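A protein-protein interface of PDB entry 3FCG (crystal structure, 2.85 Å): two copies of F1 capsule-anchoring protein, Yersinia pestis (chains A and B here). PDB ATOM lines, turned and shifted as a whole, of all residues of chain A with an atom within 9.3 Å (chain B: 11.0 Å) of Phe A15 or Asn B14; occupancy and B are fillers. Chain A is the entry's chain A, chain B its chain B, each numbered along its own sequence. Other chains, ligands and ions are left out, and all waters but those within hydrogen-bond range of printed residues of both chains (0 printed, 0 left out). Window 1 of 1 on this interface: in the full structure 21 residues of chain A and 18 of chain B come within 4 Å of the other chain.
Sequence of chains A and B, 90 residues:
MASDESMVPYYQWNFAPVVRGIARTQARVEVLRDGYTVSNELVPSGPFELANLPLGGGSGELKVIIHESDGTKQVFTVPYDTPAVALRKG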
ATOM      1  N   GLN A  12     -23.479  24.688  12.410  1.00  0.00           N
ATOM      2  CA  GLN A  12     -24.502  23.736  11.979  1.00  0.00           C
ATOM      3  C   GLN A  12     -24.013  22.785  10.886  1.00  0.00           C
ATOM      4  O   GLN A  12     -23.357  23.202   9.931  1.00  0.00           O
ATOM      5  CB  GLN A  12     -25.765  24.474  11.520  1.00  0.00           C
ATOM      6  CG  GLN A  12     -26.840  23.567  10.937  1.00  0.00           C
ATOM      7  CD  GLN A  12     -28.138  24.289  10.665  1.00  0.00           C
ATOM      8  OE1 GLN A  12     -28.446  24.622   9.519  1.00  0.00           O
ATOM      9  NE2 GLN A  12     -28.911  24.537  11.718  1.00  0.00           N
ATOM     10  N   TRP A  13     -24.350  21.506  11.042  1.00  0.00           N
ATOM     11  CA  TRP A  13     -24.009  20.476  10.069  1.00  0.00           C
ATOM     12  C   TRP A  13     -24.997  20.465   8.906  1.00  0.00           C
ATOM     13  O   TRP A  13     -26.154  20.057   9.056  1.00  0.00           O
ATOM     14  CB  TRP A  13     -23.965  19.101  10.743  1.00  0.00           C
ATOM     15  CG  TRP A  13     -22.748  18.861  11.604  1.00  0.00           C
ATOM     16  CD1 TRP A  13     -21.857  19.796  12.059  1.00  0.00           C
ATOM     17  CD2 TRP A  13     -22.312  17.603  12.138  1.00  0.00           C
ATOM     18  NE1 TRP A  13     -20.888  19.197  12.826  1.00  0.00           N
ATOM     19  CE2 TRP A  13     -21.143  17.852  12.892  1.00  0.00           C
ATOM     20  CE3 TRP A  13     -22.794  16.289  12.047  1.00  0.00           C
ATOM     21  CZ2 TRP A  13     -20.448  16.835  13.555  1.00  0.00           C
ATOM     22  CZ3 TRP A  13     -22.102  15.279  12.705  1.00  0.00           C
ATOM     23  CH2 TRP A  13     -20.941  15.559  13.448  1.00  0.00           C
ATOM     24  N   ASN A  14     -24.531  20.933   7.753  1.00  0.00           N
ATOM     25  CA  ASN A  14     -25.296  20.864   6.512  1.00  0.00           C
ATOM     26  C   ASN A  14     -24.617  19.970   5.484  1.00  0.00           C
ATOM     27  O   ASN A  14     -23.402  19.760   5.532  1.00  0.00           O
ATOM     28  CB  ASN A  14     -25.522  22.263   5.924  1.00  0.00           C
ATOM     29  CG  ASN A  14     -26.891  22.829   6.267  1.00  0.00           C
ATOM     30  OD1 ASN A  14     -27.811  22.791   5.448  1.00  0.00           O
ATOM     31  ND2 ASN A  14     -27.034  23.351   7.483  1.00  0.00           N
ATOM     32  N   PHE A  15     -25.414  19.442   4.562  1.00  0.00           N
ATOM     33  CA  PHE A  15     -24.901  18.597   3.494  1.00  0.00           C
ATOM     34  C   PHE A  15     -25.420  19.085   2.148  1.00  0.00           C
ATOM     35  O   PHE A  15     -26.624  19.068   1.889  1.00  0.00           O
ATOM     36  CB  PHE A  15     -25.270  17.128   3.736  1.00  0.00           C
ATOM     37  CG  PHE A  15     -24.654  16.541   4.980  1.00  0.00           C
ATOM     38  CD1 PHE A  15     -25.320  16.610   6.203  1.00  0.00           C
ATOM     39  CD2 PHE A  15     -23.409  15.922   4.929  1.00  0.00           C
ATOM     40  CE1 PHE A  15     -24.752  16.073   7.356  1.00  0.00           C
ATOM     41  CE2 PHE A  15     -22.834  15.380   6.076  1.00  0.00           C
ATOM     42  CZ  PHE A  15     -23.506  15.456   7.292  1.00  0.00           C
ATOM     43  N   ALA A  16     -24.499  19.539   1.303  1.00  0.00           N
ATOM     44  CA  ALA A  16     -24.846  20.095   0.001  1.00  0.00           C
ATOM     45  C   ALA A  16     -24.582  19.087  -1.113  1.00  0.00           C
ATOM     46  O   ALA A  16     -23.584  18.368  -1.074  1.00  0.00           O
ATOM     47  CB  ALA A  16     -24.076  21.385  -0.247  1.00  0.00           C
ATOM     48  N   PRO A  17     -25.481  19.026  -2.110  1.00  0.00           N
ATOM     49  CA  PRO A  17     -25.286  18.094  -3.213  1.00  0.00           C
ATOM     50  C   PRO A  17     -24.452  18.671  -4.358  1.00  0.00           C
ATOM     51  O   PRO A  17     -24.615  19.839  -4.729  1.00  0.00           O
ATOM     52  CB  PRO A  17     -26.714  17.811  -3.677  1.00  0.00           C
ATOM     53  CG  PRO A  17     -27.503  19.033  -3.301  1.00  0.00           C
ATOM     54  CD  PRO A  17     -26.729  19.799  -2.257  1.00  0.00           C
ATOM     55  N   VAL A  18     -23.560  17.848  -4.899  1.00  0.00           N
ATOM     56  CA  VAL A  18     -22.734  18.219  -6.050  1.00  0.00           C
ATOM     57  C   VAL A  18     -22.650  17.073  -7.056  1.00  0.00           C
ATOM     58  O   VAL A  18     -22.940  15.919  -6.728  1.00  0.00           O
ATOM     59  CB  VAL A  18     -21.290  18.632  -5.642  1.00  0.00           C
ATOM     60  CG1 VAL A  18     -21.279  19.993  -4.961  1.00  0.00           C
ATOM     61  CG2 VAL A  18     -20.635  17.568  -4.763  1.00  0.00           C
ATOM     62  N   VAL A  19     -22.259  17.405  -8.282  1.00  0.00           N
ATOM     63  CA  VAL A  19     -21.937  16.400  -9.289  1.00  0.00           C
ATOM     64  C   VAL A  19     -20.485  16.583  -9.743  1.00  0.00           C
ATOM     65  O   VAL A  19     -20.091  17.666 -10.185  1.00  0.00           O
ATOM     66  CB  VAL A  19     -22.953  16.389 -10.477  1.00  0.00           C
ATOM     67  CG1 VAL A  19     -23.405  17.797 -10.835  1.00  0.00           C
ATOM     68  CG2 VAL A  19     -22.378  15.670 -11.699  1.00  0.00           C
ATOM     69  N   ARG A  20     -19.698  15.519  -9.597  1.00  0.00           N
ATOM     70  CA  ARG A  20     -18.275  15.542  -9.927  1.00  0.00           C
ATOM     71  C   ARG A  20     -17.973  14.731 -11.181  1.00  0.00           C
ATOM     72  O   ARG A  20     -18.617  13.716 -11.440  1.00  0.00           O
ATOM     73  CB  ARG A  20     -17.451  15.000  -8.760  1.00  0.00           C
ATOM     74  CG  ARG A  20     -17.368  15.925  -7.558  1.00  0.00           C
ATOM     75  CD  ARG A  20     -16.575  15.287  -6.428  1.00  0.00           C
ATOM     76  NE  ARG A  20     -15.176  15.059  -6.792  1.00  0.00           N
ATOM     77  CZ  ARG A  20     -14.363  14.203  -6.175  1.00  0.00           C
ATOM     78  NH1 ARG A  20     -14.801  13.473  -5.155  1.00  0.00           N
ATOM     79  NH2 ARG A  20     -13.109  14.069  -6.586  1.00  0.00           N
ATOM     80  N   PHE A  48     -13.900  18.532 -12.229  1.00  0.00           N
ATOM     81  CA  PHE A  48     -14.827  19.625 -11.938  1.00  0.00           C
ATOM     82  C   PHE A  48     -15.841  19.249 -10.859  1.00  0.00           C
ATOM     83  O   PHE A  48     -16.152  18.072 -10.672  1.00  0.00           O
ATOM     84  CB  PHE A  48     -15.538  20.121 -13.213  1.00  0.00           C
ATOM     85  CG  PHE A  48     -16.412  19.089 -13.886  1.00  0.00           C
ATOM     86  CD1 PHE A  48     -15.960  18.404 -15.006  1.00  0.00           C
ATOM     87  CD2 PHE A  48     -17.699  18.824 -13.420  1.00  0.00           C
ATOM     88  CE1 PHE A  48     -16.767  17.461 -15.641  1.00  0.00           C
ATOM     89  CE2 PHE A  48     -18.512  17.882 -14.045  1.00  0.00           C
ATOM     90  CZ  PHE A  48     -18.045  17.200 -15.159  1.00  0.00           C
ATOM     91  N   GLU A  49     -16.347  20.258 -10.156  1.00  0.00           N
ATOM     92  CA  GLU A  49     -17.377  20.060  -9.142  1.00  0.00           C
ATOM     93  C   GLU A  49     -18.470  21.116  -9.290  1.00  0.00           C
ATOM     94  O   GLU A  49     -18.207  22.319  -9.204  1.00  0.00           O
ATOM     95  CB  GLU A  49     -16.770  20.096  -7.740  1.00  0.00           C
ATOM     96  CG  GLU A  49     -17.668  19.520  -6.656  1.00  0.00           C
ATOM     97  CD  GLU A  49     -17.028  19.570  -5.286  1.00  0.00           C
ATOM     98  OE1 GLU A  49     -16.669  18.495  -4.761  1.00  0.00           O
ATOM     99  OE2 GLU A  49     -16.878  20.682  -4.739  1.00  0.00           O
ATOM    100  N   LEU A  50     -19.695  20.651  -9.514  1.00  0.00           N
ATOM    101  CA  LEU A  50     -20.823  21.534  -9.787  1.00  0.00           C
ATOM    102  C   LEU A  50     -21.750  21.686  -8.585  1.00  0.00           C
ATOM    103  O   LEU A  50     -22.502  20.771  -8.248  1.00  0.00           O
ATOM    104  CB  LEU A  50     -21.602  21.030 -11.005  1.00  0.00           C
ATOM    105  CG  LEU A  50     -21.243  21.503 -12.419  1.00  0.00           C
ATOM    106  CD1 LEU A  50     -19.744  21.659 -12.661  1.00  0.00           C
ATOM    107  CD2 LEU A  50     -21.857  20.562 -13.438  1.00  0.00           C
ATOM    108  N   ALA A  51     -21.676  22.849  -7.942  1.00  0.00           N
ATOM    109  CA  ALA A  51     -22.575  23.204  -6.848  1.00  0.00           C
ATOM    110  C   ALA A  51     -23.807  23.916  -7.402  1.00  0.00           C
ATOM    111  O   ALA A  51     -23.864  24.219  -8.597  1.00  0.00           O
ATOM    112  CB  ALA A  51     -21.853  24.075  -5.831  1.00  0.00           C
ATOM    113  N   ASP A  81     -30.252  11.112  -5.575  1.00  0.00           N
ATOM    114  CA  ASP A  81     -31.075  10.699  -4.448  1.00  0.00           C
ATOM    115  C   ASP A  81     -30.829  11.616  -3.252  1.00  0.00           C
ATOM    116  O   ASP A  81     -29.695  12.034  -3.007  1.00  0.00           O
ATOM    117  CB  ASP A  81     -30.758   9.247  -4.071  1.00  0.00           C
ATOM    118  CG  ASP A  81     -31.678   8.705  -2.991  1.00  0.00           C
ATOM    119  OD1 ASP A  81     -32.852   9.134  -2.922  1.00  0.00           O
ATOM    120  OD2 ASP A  81     -31.223   7.840  -2.208  1.00  0.00           O
ATOM    121  N   THR A  82     -31.895  11.931  -2.520  1.00  0.00           N
ATOM    122  CA  THR A  82     -31.768  12.681  -1.273  1.00  0.00           C
ATOM    123  C   THR A  82     -31.896  11.721  -0.090  1.00  0.00           C
ATOM    124  O   THR A  82     -32.938  11.080   0.079  1.00  0.00           O
ATOM    125  CB  THR A  82     -32.806  13.818  -1.164  1.00  0.00           C
ATOM    126  OG1 THR A  82     -32.784  14.602  -2.362  1.00  0.00           O
ATOM    127  CG2 THR A  82     -32.498  14.720   0.028  1.00  0.00           C
ATOM    128  N   PRO A  83     -30.831  11.610   0.726  1.00  0.00           N
ATOM    129  CA  PRO A  83     -30.844  10.704   1.868  1.00  0.00           C
ATOM    130  C   PRO A  83     -31.617  11.280   3.052  1.00  0.00           C
ATOM    131  O   PRO A  83     -31.625  12.497   3.259  1.00  0.00           O
ATOM    132  CB  PRO A  83     -29.363  10.568   2.218  1.00  0.00           C
ATOM    133  CG  PRO A  83     -28.768  11.875   1.813  1.00  0.00           C
ATOM    134  CD  PRO A  83     -29.548  12.333   0.609  1.00  0.00           C
ATOM    135  N   ALA A  84     -32.266  10.400   3.811  1.00  0.00           N
ATOM    136  CA  ALA A  84     -32.943  10.792   5.041  1.00  0.00           C
ATOM    137  C   ALA A  84     -31.909  10.993   6.144  1.00  0.00           C
ATOM    138  O   ALA A  84     -30.986  10.188   6.295  1.00  0.00           O
ATOM    139  CB  ALA A  84     -33.963   9.742   5.444  1.00  0.00           C
ATOM    140  N   VAL A  85     -32.056  12.083   6.892  1.00  0.00           N
ATOM    141  CA  VAL A  85     -31.136  12.409   7.981  1.00  0.00           C
ATOM    142  C   VAL A  85     -31.899  12.479   9.305  1.00  0.00           C
ATOM    143  O   VAL A  85     -32.981  13.072   9.378  1.00  0.00           O
ATOM    144  CB  VAL A  85     -30.385  13.749   7.734  1.00  0.00           C
ATOM    145  CG1 VAL A  85     -29.177  13.859   8.653  1.00  0.00           C
ATOM    146  CG2 VAL A  85     -29.940  13.874   6.281  1.00  0.00           C
ATOM    147  N   ALA A  86     -31.332  11.865  10.342  1.00  0.00           N
ATOM    148  CA  ALA A  86     -31.945  11.840  11.672  1.00  0.00           C
ATOM    149  C   ALA A  86     -31.985  13.226  12.319  1.00  0.00           C
ATOM    150  O   ALA A  86     -31.130  14.075  12.055  1.00  0.00           O
ATOM    151  CB  ALA A  86     -31.215  10.855  12.572  1.00  0.00           C
ATOM    152  N   TYR B  10     -20.807  11.567 -11.333  1.00  0.00           N
ATOM    153  CA  TYR B  10     -21.603  11.014 -10.245  1.00  0.00           C
ATOM    154  C   TYR B  10     -22.134  12.088  -9.303  1.00  0.00           C
ATOM    155  O   TYR B  10     -21.500  13.125  -9.103  1.00  0.00           O
ATOM    156  CB  TYR B  10     -20.799   9.960  -9.468  1.00  0.00           C
ATOM    157  CG  TYR B  10     -19.456  10.441  -8.947  1.00  0.00           C
ATOM    158  CD1 TYR B  10     -19.302  10.834  -7.619  1.00  0.00           C
ATOM    159  CD2 TYR B  10     -18.337  10.494  -9.786  1.00  0.00           C
ATOM    160  CE1 TYR B  10     -18.071  11.274  -7.138  1.00  0.00           C
ATOM    161  CE2 TYR B  10     -17.104  10.934  -9.315  1.00  0.00           C
ATOM    162  CZ  TYR B  10     -16.980  11.322  -7.993  1.00  0.00           C
ATOM    163  OH  TYR B  10     -15.761  11.755  -7.528  1.00  0.00           O
ATOM    164  N   TYR B  11     -23.311  11.827  -8.747  1.00  0.00           N
ATOM    165  CA  TYR B  11     -23.921  12.674  -7.734  1.00  0.00           C
ATOM    166  C   TYR B  11     -23.338  12.282  -6.383  1.00  0.00           C
ATOM    167  O   TYR B  11     -23.225  11.089  -6.079  1.00  0.00           O
ATOM    168  CB  TYR B  11     -25.430  12.431  -7.721  1.00  0.00           C
ATOM    169  CG  TYR B  11     -26.275  13.568  -7.193  1.00  0.00           C
ATOM    170  CD1 TYR B  11     -26.638  14.628  -8.022  1.00  0.00           C
ATOM    171  CD2 TYR B  11     -26.746  13.566  -5.881  1.00  0.00           C
ATOM    172  CE1 TYR B  11     -27.431  15.671  -7.554  1.00  0.00           C
ATOM    173  CE2 TYR B  11     -27.543  14.607  -5.399  1.00  0.00           C
ATOM    174  CZ  TYR B  11     -27.881  15.654  -6.245  1.00  0.00           C
ATOM    175  OH  TYR B  11     -28.665  16.692  -5.794  1.00  0.00           O
ATOM    176  N   GLN B  12     -22.953  13.276  -5.585  1.00  0.00           N
ATOM    177  CA  GLN B  12     -22.498  13.018  -4.217  1.00  0.00           C
ATOM    178  C   GLN B  12     -22.820  14.154  -3.250  1.00  0.00           C
ATOM    179  O   GLN B  12     -22.998  15.302  -3.658  1.00  0.00           O
ATOM    180  CB  GLN B  12     -21.008  12.638  -4.171  1.00  0.00           C
ATOM    181  CG  GLN B  12     -20.017  13.794  -4.192  1.00  0.00           C
ATOM    182  CD  GLN B  12     -18.642  13.405  -3.650  1.00  0.00           C
ATOM    183  OE1 GLN B  12     -17.816  14.269  -3.353  1.00  0.00           O
ATOM    184  NE2 GLN B  12     -18.393  12.102  -3.520  1.00  0.00           N
ATOM    185  N   TRP B  13     -22.895  13.815  -1.966  1.00  0.00           N
ATOM    186  CA  TRP B  13     -23.224  14.779  -0.929  1.00  0.00           C
ATOM    187  C   TRP B  13     -21.986  15.172  -0.140  1.00  0.00           C
ATOM    188  O   TRP B  13     -21.354  14.334   0.503  1.00  0.00           O
ATOM    189  CB  TRP B  13     -24.309  14.219  -0.009  1.00  0.00           C
ATOM    190  CG  TRP B  13     -25.632  14.103  -0.697  1.00  0.00           C
ATOM    191  CD1 TRP B  13     -26.063  13.071  -1.480  1.00  0.00           C
ATOM    192  CD2 TRP B  13     -26.691  15.069  -0.686  1.00  0.00           C
ATOM    193  NE1 TRP B  13     -27.328  13.329  -1.950  1.00  0.00           N
ATOM    194  CE2 TRP B  13     -27.737  14.549  -1.478  1.00  0.00           C
ATOM    195  CE3 TRP B  13     -26.859  16.322  -0.079  1.00  0.00           C
ATOM    196  CZ2 TRP B  13     -28.938  15.238  -1.679  1.00  0.00           C
ATOM    197  CZ3 TRP B  13     -28.050  17.005  -0.280  1.00  0.00           C
ATOM    198  CH2 TRP B  13     -29.074  16.460  -1.075  1.00  0.00           C
ATOM    199  N   ASN B  14     -21.636  16.451  -0.216  1.00  0.00           N
ATOM    200  CA  ASN B  14     -20.501  16.995   0.519  1.00  0.00           C
ATOM    201  C   ASN B  14     -20.934  17.558   1.861  1.00  0.00           C
ATOM    202  O   ASN B  14     -21.975  18.215   1.959  1.00  0.00           O
ATOM    203  CB  ASN B  14     -19.816  18.109  -0.285  1.00  0.00           C
ATOM    204  CG  ASN B  14     -19.087  17.598  -1.516  1.00  0.00           C
ATOM    205  OD1 ASN B  14     -19.068  16.401  -1.801  1.00  0.00           O
ATOM    206  ND2 ASN B  14     -18.481  18.516  -2.256  1.00  0.00           N
ATOM    207  N   PHE B  15     -20.135  17.294   2.890  1.00  0.00           N
ATOM    208  CA  PHE B  15     -20.303  17.955   4.177  1.00  0.00           C
ATOM    209  C   PHE B  15     -19.995  19.438   3.980  1.00  0.00           C
ATOM    210  O   PHE B  15     -18.859  19.815   3.680  1.00  0.00           O
ATOM    211  CB  PHE B  15     -19.388  17.320   5.233  1.00  0.00           C
ATOM    212  CG  PHE B  15     -19.480  17.960   6.596  1.00  0.00           C
ATOM    213  CD1 PHE B  15     -20.688  18.003   7.288  1.00  0.00           C
ATOM    214  CD2 PHE B  15     -18.348  18.500   7.198  1.00  0.00           C
ATOM    215  CE1 PHE B  15     -20.771  18.590   8.551  1.00  0.00           C
ATOM    216  CE2 PHE B  15     -18.421  19.085   8.461  1.00  0.00           C
ATOM    217  CZ  PHE B  15     -19.635  19.131   9.137  1.00  0.00           C
ATOM    218  N   ALA B  16     -21.026  20.268   4.109  1.00  0.00           N
ATOM    219  CA  ALA B  16     -20.896  21.706   3.888  1.00  0.00           C
ATOM    220  C   ALA B  16     -21.486  22.487   5.061  1.00  0.00           C
ATOM    221  O   ALA B  16     -22.588  23.033   4.956  1.00  0.00           O
ATOM    222  CB  ALA B  16     -21.560  22.108   2.574  1.00  0.00           C
ATOM    223  N   PRO B  17     -20.746  22.543   6.186  1.00  0.00           N
ATOM    224  CA  PRO B  17     -21.242  23.174   7.406  1.00  0.00           C
ATOM    225  C   PRO B  17     -21.327  24.692   7.291  1.00  0.00           C
ATOM    226  O   PRO B  17     -20.630  25.295   6.465  1.00  0.00           O
ATOM    227  CB  PRO B  17     -20.196  22.784   8.446  1.00  0.00           C
ATOM    228  CG  PRO B  17     -18.947  22.603   7.665  1.00  0.00           C
ATOM    229  CD  PRO B  17     -19.380  22.014   6.362  1.00  0.00           C
ATOM    230  N   VAL B  18     -22.179  25.294   8.118  1.00  0.00           N
ATOM    231  CA  VAL B  18     -22.379  26.745   8.129  1.00  0.00           C
ATOM    232  C   VAL B  18     -22.374  27.311   9.551  1.00  0.00           C
ATOM    233  O   VAL B  18     -22.729  26.616  10.507  1.00  0.00           O
ATOM    234  CB  VAL B  18     -23.694  27.162   7.401  1.00  0.00           C
ATOM    235  CG1 VAL B  18     -23.584  26.931   5.896  1.00  0.00           C
ATOM    236  CG2 VAL B  18     -24.909  26.431   7.974  1.00  0.00           C
ATOM    237  N   ARG B  20     -24.327  29.891  11.684  1.00  0.00           N
ATOM    238  CA  ARG B  20     -25.586  30.624  11.679  1.00  0.00           C
ATOM    239  C   ARG B  20     -25.665  31.601  12.846  1.00  0.00           C
ATOM    240  O   ARG B  20     -25.035  31.392  13.886  1.00  0.00           O
ATOM    241  CB  ARG B  20     -26.777  29.663  11.713  1.00  0.00           C
ATOM    242  CG  ARG B  20     -26.947  28.839  10.447  1.00  0.00           C
ATOM    243  CD  ARG B  20     -28.273  28.102  10.446  1.00  0.00           C
ATOM    244  NE  ARG B  20     -29.400  29.003  10.203  1.00  0.00           N
ATOM    245  CZ  ARG B  20     -30.672  28.712  10.467  1.00  0.00           C
ATOM    246  NH1 ARG B  20     -31.003  27.538  10.996  1.00  0.00           N
ATOM    247  NH2 ARG B  20     -31.620  29.601  10.206  1.00  0.00           N
ATOM    248  N   GLU B  49     -26.080  33.172   7.301  1.00  0.00           N
ATOM    249  CA  GLU B  49     -25.331  31.926   7.176  1.00  0.00           C
ATOM    250  C   GLU B  49     -23.968  32.204   6.558  1.00  0.00           C
ATOM    251  O   GLU B  49     -23.854  33.011   5.630  1.00  0.00           O
ATOM    252  CB  GLU B  49     -26.083  30.921   6.304  1.00  0.00           C
ATOM    253  CG  GLU B  49     -27.251  30.236   6.986  1.00  0.00           C
ATOM    254  CD  GLU B  49     -27.648  28.935   6.307  1.00  0.00           C
ATOM    255  OE1 GLU B  49     -27.320  28.748   5.113  1.00  0.00           O
ATOM    256  OE2 GLU B  49     -28.292  28.095   6.972  1.00  0.00           O
ATOM    257  N   ALA B  51     -21.069  30.219   4.657  1.00  0.00           N
ATOM    258  CA  ALA B  51     -20.751  28.957   3.978  1.00  0.00           C
ATOM    259  C   ALA B  51     -19.294  28.854   3.513  1.00  0.00           C
ATOM    260  O   ALA B  51     -18.513  29.797   3.669  1.00  0.00           O
ATOM    261  CB  ALA B  51     -21.708  28.734   2.803  1.00  0.00           C
ATOM    262  N   ASN B  52     -18.946  27.690   2.961  1.00  0.00           N
ATOM    263  CA  ASN B  52     -17.640  27.423   2.344  1.00  0.00           C
ATOM    264  C   ASN B  52     -16.441  27.967   3.126  1.00  0.00           C
ATOM    265  O   ASN B  52     -15.631  28.732   2.596  1.00  0.00           O
ATOM    266  CB  ASN B  52     -17.620  27.922   0.890  1.00  0.00           C
ATOM    267  CG  ASN B  52     -18.667  27.238   0.019  1.00  0.00           C
ATOM    268  OD1 ASN B  52     -18.664  26.015  -0.137  1.00  0.00           O
ATOM    269  ND2 ASN B  52     -19.566  28.031  -0.557  1.00  0.00           N
ATOM    270  N   ASP B  81     -17.158  20.859  14.976  1.00  0.00           N
ATOM    271  CA  ASP B  81     -16.770  19.454  14.906  1.00  0.00           C
ATOM    272  C   ASP B  81     -17.039  18.878  13.519  1.00  0.00           C
ATOM    273  O   ASP B  81     -17.901  19.366  12.786  1.00  0.00           O
ATOM    274  CB  ASP B  81     -17.510  18.644  15.980  1.00  0.00           C
ATOM    275  CG  ASP B  81     -16.803  17.341  16.334  1.00  0.00           C
ATOM    276  OD1 ASP B  81     -15.656  17.121  15.883  1.00  0.00           O
ATOM    277  OD2 ASP B  81     -17.402  16.533  17.075  1.00  0.00           O
ATOM    278  N   THR B  82     -16.293  17.834  13.172  1.00  0.00           N
ATOM    279  CA  THR B  82     -16.399  17.189  11.870  1.00  0.00           C
ATOM    280  C   THR B  82     -16.665  15.692  12.071  1.00  0.00           C
ATOM    281  O   THR B  82     -15.916  15.028  12.792  1.00  0.00           O
ATOM    282  CB  THR B  82     -15.104  17.391  11.046  1.00  0.00           C
ATOM    283  OG1 THR B  82     -14.541  18.677  11.339  1.00  0.00           O
ATOM    284  CG2 THR B  82     -15.384  17.293   9.553  1.00  0.00           C
ATOM    285  N   PRO B  83     -17.734  15.161  11.443  1.00  0.00           N
ATOM    286  CA  PRO B  83     -18.078  13.743  11.591  1.00  0.00           C
ATOM    287  C   PRO B  83     -17.029  12.821  10.979  1.00  0.00           C
ATOM    288  O   PRO B  83     -16.401  13.175   9.980  1.00  0.00           O
ATOM    289  CB  PRO B  83     -19.402  13.614  10.831  1.00  0.00           C
ATOM    290  CG  PRO B  83     -19.414  14.747   9.880  1.00  0.00           C
ATOM    291  CD  PRO B  83     -18.681  15.864  10.560  1.00  0.00           C
ATOM    292  N   ALA B  84     -16.844  11.651  11.584  1.00  0.00           N
ATOM    293  CA  ALA B  84     -15.873  10.674  11.104  1.00  0.00           C
ATOM    294  C   ALA B  84     -16.506   9.723  10.088  1.00  0.00           C
ATOM    295  O   ALA B  84     -17.546   9.118  10.354  1.00  0.00           O
ATOM    296  CB  ALA B  84     -15.275   9.899  12.269  1.00  0.00           C
ATOM    297  N   VAL B  85     -15.872   9.615   8.923  1.00  0.00           N
ATOM    298  CA  VAL B  85     -16.344   8.750   7.840  1.00  0.00           C
ATOM    299  C   VAL B  85     -15.207   7.845   7.359  1.00  0.00           C
ATOM    300  O   VAL B  85     -15.363   6.626   7.267  1.00  0.00           O
ATOM    301  CB  VAL B  85     -16.907   9.572   6.647  1.00  0.00           C
ATOM    302  CG1 VAL B  85     -17.261   8.665   5.474  1.00  0.00           C
ATOM    303  CG2 VAL B  85     -18.128  10.382   7.071  1.00  0.00           C
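Gln A12 touches Pro B17, and with the chains exchanged Pro A17 touches Gln B12.
Trp A13 touches Phe B15, and with the chains exchanged Phe A15 touches Trp B13.
Phe B15 touches its own counterpart, Phe A15.
Pro A17 touches Trp B13, but with the chains exchanged Trp A13 does not touch Pro B17 (4.7 Å).
The side-chain amide oxygen (OE1) of Gln A12 sits at hydrogen-bond distance from the side-chain amide nitrogen (ND2) of Asn A14 (2.8 Å).
The guanidinium group of Arg B20 lies within salt-bridge range of the side-chain carboxylate of Glu B49 (3.5 Å).
OD1 of Asn B14 sits close to OE1 of Gln B12.
O of Val A19 is in hydrogen-bond range of N of Leu A50 (3.1 Å).
The backbone NH (N) of Asn B14 lies within hydrogen-bond range of the backbone carbonyl oxygen (O) of Ala A16, 2.9 Å away.
The backbone carbonyl oxygen (O) of Tyr B10 lies within hydrogen-bond range of the backbone NH (N) of Arg A20.
The backbone NH (N) of Gln A12 is in hydrogen-bond range of the backbone carbonyl oxygen (O) of Val B18 (2.8 Å).
The side-chain carboxylate of Glu A49 lies within hydrogen-bond range of the side-chain amide nitrogen of Asn B14 (3.1 Å).
The backbone NH (N) of Ala B16 is in hydrogen-bond range of the backbone carbonyl oxygen (O) of Asn A14, 2.8 Å away.
The indole nitrogen of Trp A13 is in hydrogen-bond range of the backbone carbonyl oxygen of Asp B81 (3.0 Å).
The backbone carbonyl oxygen (O) of Asp A81 is in hydrogen-bond range of the indole nitrogen (NE1) of Trp B13 (2.9 Å).
The backbone carbonyl oxygen (O) of Val A18 is in hydrogen-bond range of the backbone NH (N) of Gln B12 (2.9 Å).
Printed residues of chain A that touch a printed residue of chain B: Gln A12, Trp A13, Asn A14, Phe A15, Ala A16, Pro A17, Val A18, Val A19, Arg A20, Glu A49, Asp A81, Thr A82 and Pro A83.
Among the printed residues, 30 pairs touch across the chains.
Among the printed residues, no Asp or Glu carboxylate lies within 4 Å of a Lys or Arg side-chain nitrogen of the other chain.
Printed residues of chain B within 4 Å of Gln A12: Pro B17, Val B18 and Arg B20.
Phe A15 touches just these residues of chain B: Trp B13 (3.3 Å), Asn B14 (3.3 Å) and Phe B15 (3.6 Å).
Ala A16 touches three residues of chain B.
Of the printed residues of chain A, Tyr B11 touches Pro A17 (3.1 Å) and Val A18 (3.5 Å).
Asn B14 touches just these residues of chain A: Phe A15 (3.3 Å), Ala A16 (2.9 Å), Val A18 (3.4 Å) and Glu A49 (3.1 Å).
Ala B16 touches just these residues of chain A: Asn A14 (2.8 Å) and Ala A16 (3.8 Å).
Val B85 touches none of the printed residues of chain A.
The nearest residue of chain A that does not touch Asn B14 is Asn A14 (4.1 Å).
The nearest printed residue of chain B that does not touch Glu A49 is Gln B12 (4.6 Å).
Among the printed residues, pairs that only touch across the chains: Pro A17 with Tyr B11, Gln A12 with Pro B17, Val A19 with Tyr B10, Phe A15 with Trp B13, Phe A15 with Asn B14, Val A18 with Asn B14, Arg A20 with Gln B12, Pro A83 with Trp B13, Val A18 with Tyr B11, Phe A15 with Phe B15, Gln A12 with Arg B20, Trp A13 with Pro B83, Ala A16 with Trp B13, Pro A17 with Gln B12, Trp A13 with Phe B15, Pro A17 with Trp B13, Asn A14 with Phe B15, Asn A14 with Val B18, Thr A82 with Trp B13, Ala A16 with Ala B16, Asn A14 with Pro B17 and Val A18 with Tyr B10.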
